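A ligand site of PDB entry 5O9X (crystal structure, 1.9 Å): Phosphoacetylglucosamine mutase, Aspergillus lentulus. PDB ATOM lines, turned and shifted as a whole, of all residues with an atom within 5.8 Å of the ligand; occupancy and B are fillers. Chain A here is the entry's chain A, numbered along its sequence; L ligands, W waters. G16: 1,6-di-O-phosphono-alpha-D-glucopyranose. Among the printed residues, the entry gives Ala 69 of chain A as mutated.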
ATOM      1  N   THR A  29     -14.702   2.501   6.750  1.00  0.00           N
ATOM      2  CA  THR A  29     -14.346   3.892   6.455  1.00  0.00           C
ATOM      3  C   THR A  29     -15.595   4.786   6.542  1.00  0.00           C
ATOM      4  O   THR A  29     -15.491   5.964   7.006  1.00  0.00           O
ATOM      5  CB  THR A  29     -13.763   3.928   5.028  1.00  0.00           C
ATOM      6  OG1 THR A  29     -12.592   3.103   4.997  1.00  0.00           O
ATOM      7  CG2 THR A  29     -13.313   5.340   4.628  1.00  0.00           C
ATOM      8  N   ALA A  30     -16.710   4.310   5.972  1.00  0.00           N
ATOM      9  CA  ALA A  30     -17.952   5.125   5.812  1.00  0.00           C
ATOM     10  C   ALA A  30     -19.246   4.453   6.313  1.00  0.00           C
ATOM     11  O   ALA A  30     -20.330   4.904   5.961  1.00  0.00           O
ATOM     12  CB  ALA A  30     -18.131   5.523   4.323  1.00  0.00           C
ATOM     13  N   ARG A  33     -20.829  -1.908   5.088  1.00  0.00           N
ATOM     14  CA  ARG A  33     -20.921  -2.087   3.658  1.00  0.00           C
ATOM     15  C   ARG A  33     -20.479  -3.495   3.298  1.00  0.00           C
ATOM     16  O   ARG A  33     -19.408  -3.934   3.715  1.00  0.00           O
ATOM     17  CB  ARG A  33     -19.981  -1.045   2.997  1.00  0.00           C
ATOM     18  CG  ARG A  33     -20.320  -0.881   1.535  1.00  0.00           C
ATOM     19  CD  ARG A  33     -19.495   0.292   1.010  1.00  0.00           C
ATOM     20  NE  ARG A  33     -19.902   1.621   1.468  1.00  0.00           N
ATOM     21  CZ  ARG A  33     -19.314   2.747   0.944  1.00  0.00           C
ATOM     22  NH1 ARG A  33     -18.455   2.634  -0.115  1.00  0.00           N
ATOM     23  NH2 ARG A  33     -19.661   3.987   1.331  1.00  0.00           N
ATOM     24  N   ALA A  68     -24.198   1.671  -0.964  1.00  0.00           N
ATOM     25  CA  ALA A  68     -22.765   1.310  -0.974  1.00  0.00           C
ATOM     26  C   ALA A  68     -21.940   2.211  -1.947  1.00  0.00           C
ATOM     27  O   ALA A  68     -20.785   1.877  -2.234  1.00  0.00           O
ATOM     28  CB  ALA A  68     -22.556  -0.184  -1.238  1.00  0.00           C
ATOM     29  N   ALA A  69     -22.517   3.351  -2.417  1.00  0.00           N
ATOM     30  CA  ALA A  69     -21.701   4.487  -3.035  1.00  0.00           C
ATOM     31  C   ALA A  69     -20.882   4.045  -4.278  1.00  0.00           C
ATOM     32  O   ALA A  69     -21.497   3.687  -5.281  1.00  0.00           O
ATOM     33  CB  ALA A  69     -20.805   5.071  -1.966  1.00  0.00           C
ATOM     34  N   HIS A  70     -19.522   3.954  -4.214  1.00  0.00           N
ATOM     35  CA  HIS A  70     -18.713   3.559  -5.370  1.00  0.00           C
ATOM     36  C   HIS A  70     -18.713   2.036  -5.620  1.00  0.00           C
ATOM     37  O   HIS A  70     -18.257   1.579  -6.704  1.00  0.00           O
ATOM     38  CB  HIS A  70     -17.200   3.993  -5.201  1.00  0.00           C
ATOM     39  CG  HIS A  70     -16.382   3.049  -4.405  1.00  0.00           C
ATOM     40  ND1 HIS A  70     -16.298   3.121  -3.018  1.00  0.00           N
ATOM     41  CD2 HIS A  70     -15.616   1.981  -4.764  1.00  0.00           C
ATOM     42  CE1 HIS A  70     -15.505   2.158  -2.579  1.00  0.00           C
ATOM     43  NE2 HIS A  70     -15.087   1.450  -3.622  1.00  0.00           N
ATOM     44  N   ASN A  71     -19.144   1.262  -4.614  1.00  0.00           N
ATOM     45  CA  ASN A  71     -19.093  -0.243  -4.692  1.00  0.00           C
ATOM     46  C   ASN A  71     -19.912  -0.859  -5.854  1.00  0.00           C
ATOM     47  O   ASN A  71     -20.895  -0.261  -6.352  1.00  0.00           O
ATOM     48  CB  ASN A  71     -19.534  -0.933  -3.388  1.00  0.00           C
ATOM     49  CG  ASN A  71     -18.495  -0.728  -2.250  1.00  0.00           C
ATOM     50  OD1 ASN A  71     -17.941   0.354  -2.097  1.00  0.00           O
ATOM     51  ND2 ASN A  71     -18.284  -1.777  -1.452  1.00  0.00           N
ATOM     52  N   ASP A 284     -20.218   9.401  -9.135  1.00  0.00           N
ATOM     53  CA  ASP A 284     -20.361   7.956  -8.846  1.00  0.00           C
ATOM     54  C   ASP A 284     -21.824   7.623  -8.570  1.00  0.00           C
ATOM     55  O   ASP A 284     -22.693   8.484  -8.751  1.00  0.00           O
ATOM     56  CB  ASP A 284     -19.340   7.457  -7.776  1.00  0.00           C
ATOM     57  CG  ASP A 284     -19.643   7.992  -6.425  1.00  0.00           C
ATOM     58  OD1 ASP A 284     -20.459   8.974  -6.325  1.00  0.00           O
ATOM     59  OD2 ASP A 284     -19.066   7.448  -5.425  1.00  0.00           O
ATOM     60  N   ASP A 286     -23.807   7.121  -5.938  1.00  0.00           N
ATOM     61  CA  ASP A 286     -24.661   7.947  -5.007  1.00  0.00           C
ATOM     62  C   ASP A 286     -24.413   9.485  -5.154  1.00  0.00           C
ATOM     63  O   ASP A 286     -24.825  10.324  -4.314  1.00  0.00           O
ATOM     64  CB  ASP A 286     -24.523   7.527  -3.537  1.00  0.00           C
ATOM     65  CG  ASP A 286     -23.148   7.826  -2.949  1.00  0.00           C
ATOM     66  OD1 ASP A 286     -22.225   7.941  -3.779  1.00  0.00           O
ATOM     67  OD2 ASP A 286     -22.974   7.906  -1.664  1.00  0.00           O
ATOM     68  N   ASP A 288     -21.629  11.236  -4.788  1.00  0.00           N
ATOM     69  CA  ASP A 288     -20.858  11.908  -3.799  1.00  0.00           C
ATOM     70  C   ASP A 288     -19.353  11.957  -4.090  1.00  0.00           C
ATOM     71  O   ASP A 288     -18.528  12.245  -3.199  1.00  0.00           O
ATOM     72  CB  ASP A 288     -21.174  11.325  -2.426  1.00  0.00           C
ATOM     73  CG  ASP A 288     -21.023  12.393  -1.328  1.00  0.00           C
ATOM     74  OD1 ASP A 288     -21.090  13.627  -1.630  1.00  0.00           O
ATOM     75  OD2 ASP A 288     -20.745  11.975  -0.229  1.00  0.00           O
ATOM     76  N   ARG A 289     -19.016  11.689  -5.333  1.00  0.00           N
ATOM     77  CA  ARG A 289     -17.652  11.908  -5.856  1.00  0.00           C
ATOM     78  C   ARG A 289     -17.812  12.552  -7.215  1.00  0.00           C
ATOM     79  O   ARG A 289     -18.746  12.188  -7.965  1.00  0.00           O
ATOM     80  CB  ARG A 289     -16.937  10.568  -6.117  1.00  0.00           C
ATOM     81  CG  ARG A 289     -16.639   9.790  -4.847  1.00  0.00           C
ATOM     82  CD  ARG A 289     -15.867   8.531  -5.264  1.00  0.00           C
ATOM     83  NE  ARG A 289     -15.705   7.625  -4.101  1.00  0.00           N
ATOM     84  CZ  ARG A 289     -14.897   6.567  -4.119  1.00  0.00           C
ATOM     85  NH1 ARG A 289     -14.229   6.273  -5.231  1.00  0.00           N
ATOM     86  NH2 ARG A 289     -14.822   5.751  -3.100  1.00  0.00           N
ATOM     87  N   TYR A 339      -3.277   9.488  -0.840  1.00  0.00           N
ATOM     88  CA  TYR A 339      -3.562   9.134  -2.236  1.00  0.00           C
ATOM     89  C   TYR A 339      -3.361  10.366  -3.131  1.00  0.00           C
ATOM     90  O   TYR A 339      -3.428  10.217  -4.374  1.00  0.00           O
ATOM     91  CB  TYR A 339      -5.039   8.674  -2.369  1.00  0.00           C
ATOM     92  CG  TYR A 339      -5.201   7.282  -1.768  1.00  0.00           C
ATOM     93  CD1 TYR A 339      -4.697   6.173  -2.444  1.00  0.00           C
ATOM     94  CD2 TYR A 339      -5.700   7.123  -0.488  1.00  0.00           C
ATOM     95  CE1 TYR A 339      -4.779   4.912  -1.918  1.00  0.00           C
ATOM     96  CE2 TYR A 339      -5.821   5.835   0.064  1.00  0.00           C
ATOM     97  CZ  TYR A 339      -5.298   4.761  -0.659  1.00  0.00           C
ATOM     98  OH  TYR A 339      -5.310   3.484  -0.110  1.00  0.00           O
ATOM     99  N   THR A 361      -7.604   8.302   5.294  1.00  0.00           N
ATOM    100  CA  THR A 361      -8.668   8.175   4.318  1.00  0.00           C
ATOM    101  C   THR A 361     -10.031   8.201   5.004  1.00  0.00           C
ATOM    102  O   THR A 361     -10.216   7.600   6.099  1.00  0.00           O
ATOM    103  CB  THR A 361      -8.464   6.896   3.502  1.00  0.00           C
ATOM    104  OG1 THR A 361      -7.472   7.190   2.530  1.00  0.00           O
ATOM    105  CG2 THR A 361      -9.721   6.448   2.765  1.00  0.00           C
ATOM    106  N   GLY A 362     -10.957   8.906   4.367  1.00  0.00           N
ATOM    107  CA  GLY A 362     -12.371   8.919   4.873  1.00  0.00           C
ATOM    108  C   GLY A 362     -12.696  10.401   5.186  1.00  0.00           C
ATOM    109  O   GLY A 362     -12.025  11.038   6.001  1.00  0.00           O
ATOM    110  N   VAL A 363     -13.770  10.910   4.588  1.00  0.00           N
ATOM    111  CA  VAL A 363     -14.221  12.308   4.740  1.00  0.00           C
ATOM    112  C   VAL A 363     -14.276  12.822   6.227  1.00  0.00           C
ATOM    113  O   VAL A 363     -13.928  13.945   6.533  1.00  0.00           O
ATOM    114  CB  VAL A 363     -15.675  12.475   4.121  1.00  0.00           C
ATOM    115  CG1 VAL A 363     -16.164  13.920   4.262  1.00  0.00           C
ATOM    116  CG2 VAL A 363     -15.643  12.139   2.646  1.00  0.00           C
ATOM    117  N   GLU A 380     -10.475  14.267  -1.440  1.00  0.00           N
ATOM    118  CA  GLU A 380      -9.688  13.098  -1.659  1.00  0.00           C
ATOM    119  C   GLU A 380      -9.494  13.029  -3.139  1.00  0.00           C
ATOM    120  O   GLU A 380     -10.345  13.577  -3.887  1.00  0.00           O
ATOM    121  CB  GLU A 380     -10.453  11.853  -1.136  1.00  0.00           C
ATOM    122  CG  GLU A 380     -10.550  11.949   0.397  1.00  0.00           C
ATOM    123  CD  GLU A 380     -11.276  10.743   0.972  1.00  0.00           C
ATOM    124  OE1 GLU A 380     -12.526  10.687   0.913  1.00  0.00           O
ATOM    125  OE2 GLU A 380     -10.601   9.856   1.479  1.00  0.00           O
ATOM    126  N   ASN A 382     -10.029  10.744  -5.124  1.00  0.00           N
ATOM    127  CA  ASN A 382     -11.136  10.026  -5.770  1.00  0.00           C
ATOM    128  C   ASN A 382     -12.318  10.962  -6.073  1.00  0.00           C
ATOM    129  O   ASN A 382     -13.318  10.521  -6.667  1.00  0.00           O
ATOM    130  CB  ASN A 382     -11.631   8.834  -4.875  1.00  0.00           C
ATOM    131  CG  ASN A 382     -12.196   9.278  -3.517  1.00  0.00           C
ATOM    132  OD1 ASN A 382     -12.723  10.363  -3.401  1.00  0.00           O
ATOM    133  ND2 ASN A 382     -12.107   8.411  -2.505  1.00  0.00           N
ATOM    134  N   HIS A 384     -14.200  12.941  -3.690  1.00  0.00           N
ATOM    135  CA  HIS A 384     -14.924  13.461  -2.506  1.00  0.00           C
ATOM    136  C   HIS A 384     -14.368  14.760  -2.054  1.00  0.00           C
ATOM    137  O   HIS A 384     -13.128  14.965  -2.082  1.00  0.00           O
ATOM    138  CB  HIS A 384     -14.696  12.497  -1.334  1.00  0.00           C
ATOM    139  CG  HIS A 384     -15.762  11.493  -1.208  1.00  0.00           C
ATOM    140  ND1 HIS A 384     -17.020  11.806  -0.676  1.00  0.00           N
ATOM    141  CD2 HIS A 384     -15.804  10.182  -1.545  1.00  0.00           C
ATOM    142  CE1 HIS A 384     -17.758  10.699  -0.643  1.00  0.00           C
ATOM    143  NE2 HIS A 384     -17.046   9.698  -1.169  1.00  0.00           N
ATOM    144  N   ARG A 505      -2.580  -0.199   2.297  1.00  0.00           N
ATOM    145  CA  ARG A 505      -3.403  -0.142   3.516  1.00  0.00           C
ATOM    146  C   ARG A 505      -4.680  -0.907   3.173  1.00  0.00           C
ATOM    147  O   ARG A 505      -5.092  -0.994   1.984  1.00  0.00           O
ATOM    148  CB  ARG A 505      -3.816   1.267   3.951  1.00  0.00           C
ATOM    149  CG  ARG A 505      -4.384   2.127   2.792  1.00  0.00           C
ATOM    150  CD  ARG A 505      -4.945   3.492   3.288  1.00  0.00           C
ATOM    151  NE  ARG A 505      -6.259   3.357   3.940  1.00  0.00           N
ATOM    152  CZ  ARG A 505      -7.437   3.186   3.289  1.00  0.00           C
ATOM    153  NH1 ARG A 505      -7.513   3.064   1.955  1.00  0.00           N
ATOM    154  NH2 ARG A 505      -8.556   3.118   3.994  1.00  0.00           N
ATOM    155  N   ALA A 506      -5.269  -1.469   4.219  1.00  0.00           N
ATOM    156  CA  ALA A 506      -6.562  -2.208   4.114  1.00  0.00           C
ATOM    157  C   ALA A 506      -7.636  -1.189   3.756  1.00  0.00           C
ATOM    158  O   ALA A 506      -7.695  -0.042   4.287  1.00  0.00           O
ATOM    159  CB  ALA A 506      -6.908  -2.851   5.482  1.00  0.00           C
ATOM    160  N   SER A 507      -8.481  -1.582   2.787  1.00  0.00           N
ATOM    161  CA  SER A 507      -9.704  -0.844   2.523  1.00  0.00           C
ATOM    162  C   SER A 507     -10.675  -1.059   3.686  1.00  0.00           C
ATOM    163  O   SER A 507     -10.734  -2.192   4.235  1.00  0.00           O
ATOM    164  CB  SER A 507     -10.332  -1.385   1.194  1.00  0.00           C
ATOM    165  OG  SER A 507     -11.645  -0.845   1.033  1.00  0.00           O
ATOM    166  N   GLY A 508     -11.454  -0.015   3.994  1.00  0.00           N
ATOM    167  CA  GLY A 508     -12.613  -0.073   4.936  1.00  0.00           C
ATOM    168  C   GLY A 508     -13.921  -0.019   4.230  1.00  0.00           C
ATOM    169  O   GLY A 508     -14.979   0.228   4.899  1.00  0.00           O
ATOM    170  N   THR A 509     -13.936  -0.209   2.886  1.00  0.00           N
ATOM    171  CA  THR A 509     -15.231  -0.265   2.149  1.00  0.00           C
ATOM    172  C   THR A 509     -15.402  -1.599   1.370  1.00  0.00           C
ATOM    173  O   THR A 509     -16.522  -1.935   0.955  1.00  0.00           O
ATOM    174  CB  THR A 509     -15.440   0.903   1.153  1.00  0.00           C
ATOM    175  OG1 THR A 509     -14.427   0.863   0.121  1.00  0.00           O
ATOM    176  CG2 THR A 509     -15.424   2.270   1.839  1.00  0.00           C
ATOM    177  N   GLU A 510     -14.283  -2.290   1.073  1.00  0.00           N
ATOM    178  CA  GLU A 510     -14.223  -3.512   0.332  1.00  0.00           C
ATOM    179  C   GLU A 510     -13.211  -4.438   0.986  1.00  0.00           C
ATOM    180  O   GLU A 510     -12.309  -3.969   1.691  1.00  0.00           O
ATOM    181  CB  GLU A 510     -13.651  -3.227  -1.086  1.00  0.00           C
ATOM    182  CG  GLU A 510     -14.550  -2.335  -1.888  1.00  0.00           C
ATOM    183  CD  GLU A 510     -13.877  -2.021  -3.217  1.00  0.00           C
ATOM    184  OE1 GLU A 510     -13.629  -0.815  -3.568  1.00  0.00           O
ATOM    185  OE2 GLU A 510     -13.579  -3.032  -3.846  1.00  0.00           O
ATOM    186  N   ARG A 514      -5.282  -1.873  -0.618  1.00  0.00           N
ATOM    187  CA  ARG A 514      -4.977  -0.974  -1.739  1.00  0.00           C
ATOM    188  C   ARG A 514      -3.510  -0.655  -1.787  1.00  0.00           C
ATOM    189  O   ARG A 514      -2.929  -0.340  -0.756  1.00  0.00           O
ATOM    190  CB  ARG A 514      -5.742   0.362  -1.557  1.00  0.00           C
ATOM    191  CG  ARG A 514      -7.254   0.190  -1.495  1.00  0.00           C
ATOM    192  CD  ARG A 514      -7.992   1.525  -1.747  1.00  0.00           C
ATOM    193  NE  ARG A 514      -9.464   1.399  -1.510  1.00  0.00           N
ATOM    194  CZ  ARG A 514     -10.315   0.762  -2.335  1.00  0.00           C
ATOM    195  NH1 ARG A 514      -9.840   0.112  -3.441  1.00  0.00           N
ATOM    196  NH2 ARG A 514     -11.648   0.747  -2.025  1.00  0.00           N
HETATM  197  C1  G16 L   1     -15.786   5.997   0.929  1.00  0.00           C
HETATM  198  C2  G16 L   1     -15.387   7.155   1.841  1.00  0.00           C
HETATM  199  C3  G16 L   1     -14.151   7.899   1.246  1.00  0.00           C
HETATM  200  C4  G16 L   1     -12.963   6.998   0.958  1.00  0.00           C
HETATM  201  C5  G16 L   1     -13.422   5.880   0.040  1.00  0.00           C
HETATM  202  C6  G16 L   1     -12.445   4.729  -0.108  1.00  0.00           C
HETATM  203  O1  G16 L   1     -16.188   6.526  -0.341  1.00  0.00           O
HETATM  204  O2  G16 L   1     -16.471   8.083   2.122  1.00  0.00           O
HETATM  205  O3  G16 L   1     -13.872   8.939   2.082  1.00  0.00           O
HETATM  206  O4  G16 L   1     -11.811   7.670   0.274  1.00  0.00           O
HETATM  207  O5  G16 L   1     -14.550   5.155   0.600  1.00  0.00           O
HETATM  208  O6  G16 L   1     -12.224   4.168   1.261  1.00  0.00           O
HETATM  209  P   G16 L   1     -11.288   2.851   1.407  1.00  0.00           P
HETATM  210  O1P G16 L   1      -9.955   3.096   0.672  1.00  0.00           O
HETATM  211  O2P G16 L   1     -12.023   1.678   0.716  1.00  0.00           O
HETATM  212  O3P G16 L   1     -11.172   2.516   2.914  1.00  0.00           O
HETATM  213  P'  G16 L   1     -17.689   6.302  -0.970  1.00  0.00           P
HETATM  214  O1X G16 L   1     -18.695   6.298   0.201  1.00  0.00           O
HETATM  215  O2X G16 L   1     -17.715   4.854  -1.565  1.00  0.00           O
HETATM  216  O3X G16 L   1     -17.872   7.264  -2.090  1.00  0.00           O
HETATM  217  O   HOH W   1     -20.858   8.043   0.107  1.00  0.00           O
HETATM  218  O   HOH W   2      -9.048   4.930  -1.170  1.00  0.00           O
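The guanidinium group (NH2) of Arg 33 lies within salt-bridge range of an oxygen (O1X) of the ligand, 2.7 Å away.
An oxygen (O4) of the ligand sits at hydrogen-bond distance from the side-chain amide nitrogen of Asn 382 (2.9 Å).
The side-chain hydroxyl (OG1) of Thr 509 lies within hydrogen-bond range of an oxygen (O2P) of the ligand (2.6 Å).
The guanidinium group (NH1) of Arg 505 is in salt-bridge range of an oxygen (O1P) of the ligand (2.8 Å).
O3 of the ligand lies within hydrogen-bond range of N of Val 363, at 3.2 Å.
An oxygen (O3P) of the ligand is in hydrogen-bond range of the backbone NH (N) of Gly 508, at 2.8 Å.
The side-chain hydroxyl of Thr 29 lies within hydrogen-bond range of an oxygen (O3P) of the ligand (2.6 Å).
An oxygen (O2P) of the ligand lies within hydrogen-bond range of the backbone NH (N) of Thr 509.
The side-chain carboxylate (OE1) of Glu 380 sits at hydrogen-bond distance from an oxygen (O3) of the ligand.
A ring nitrogen (NE2) of His 384 lies within hydrogen-bond range of an oxygen (O3X) of the ligand (2.7 Å).
An oxygen (O1P) of the ligand is in salt-bridge range of the guanidinium group (NE) of Arg 514, 2.8 Å away.
ND1 of His 70 is in hydrogen-bond range of O2X of the ligand (2.7 Å).
The backbone NH of His 70 lies within hydrogen-bond range of an oxygen (O2X) of the ligand, 3.3 Å away.
An oxygen (O2P) of the ligand lies within hydrogen-bond range of the side-chain hydroxyl (OG) of Ser 507 (2.6 Å).
The guanidinium group (NE) of Arg 289 lies within salt-bridge range of an oxygen (O3X) of the ligand, at 3.0 Å.
O of Thr 509 is in hydrogen-bond range of ND2 of Asn 71, at 3.0 Å.
The side-chain hydroxyl (OG) of Ser 507 is in hydrogen-bond range of the guanidinium group (NH2) of Arg 514 (3.4 Å).
The side-chain hydroxyl of Ser 507 lies within hydrogen-bond range of the backbone NH of Glu 510 (3.0 Å).
OD1 of Asn 382 lies within hydrogen-bond range of N of His 384.
NH2 of Arg 514 lies within salt-bridge range of OE1 of Glu 510.
ND1 of His 384 is in hydrogen-bond range of O of Asp 288, at 3.0 Å.
NE2 of His 70 lies within hydrogen-bond range of OE1 of Glu 510 (2.7 Å).
The backbone NH (N) of Gly 362 lies within hydrogen-bond range of the side-chain carboxylate (OE2) of Glu 380, 3.1 Å away.
Ala 30 touches the ligand.
Ala 69 touches the ligand.
Asp 284 touches the ligand (OD2 to O3X, 3.5 Å).
Thr 361 touches the ligand (CG2 to O4, 3.5 Å).
CA of Gly 362 touches O3 of the ligand, at 3.2 Å.
Hydrophobic or aromatic side chains that line the ligand: Ala 30, Ala 69, His 70, Val 363 and His 384.
18 residues have an atom within 4 Å of the ligand: Thr 29, Ala 30, Arg 33, Ala 69, His 70, Asp 284, Arg 289, Thr 361, Gly 362, Val 363, Glu 380, Asn 382, His 384, Arg 505, Ser 507, Gly 508, Thr 509 and Arg 514.
Water W1 bridges the side-chain carboxylate (OD2) of Asp 286 (2.8 Å) and an oxygen (O1X) of the ligand (2.8 Å).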
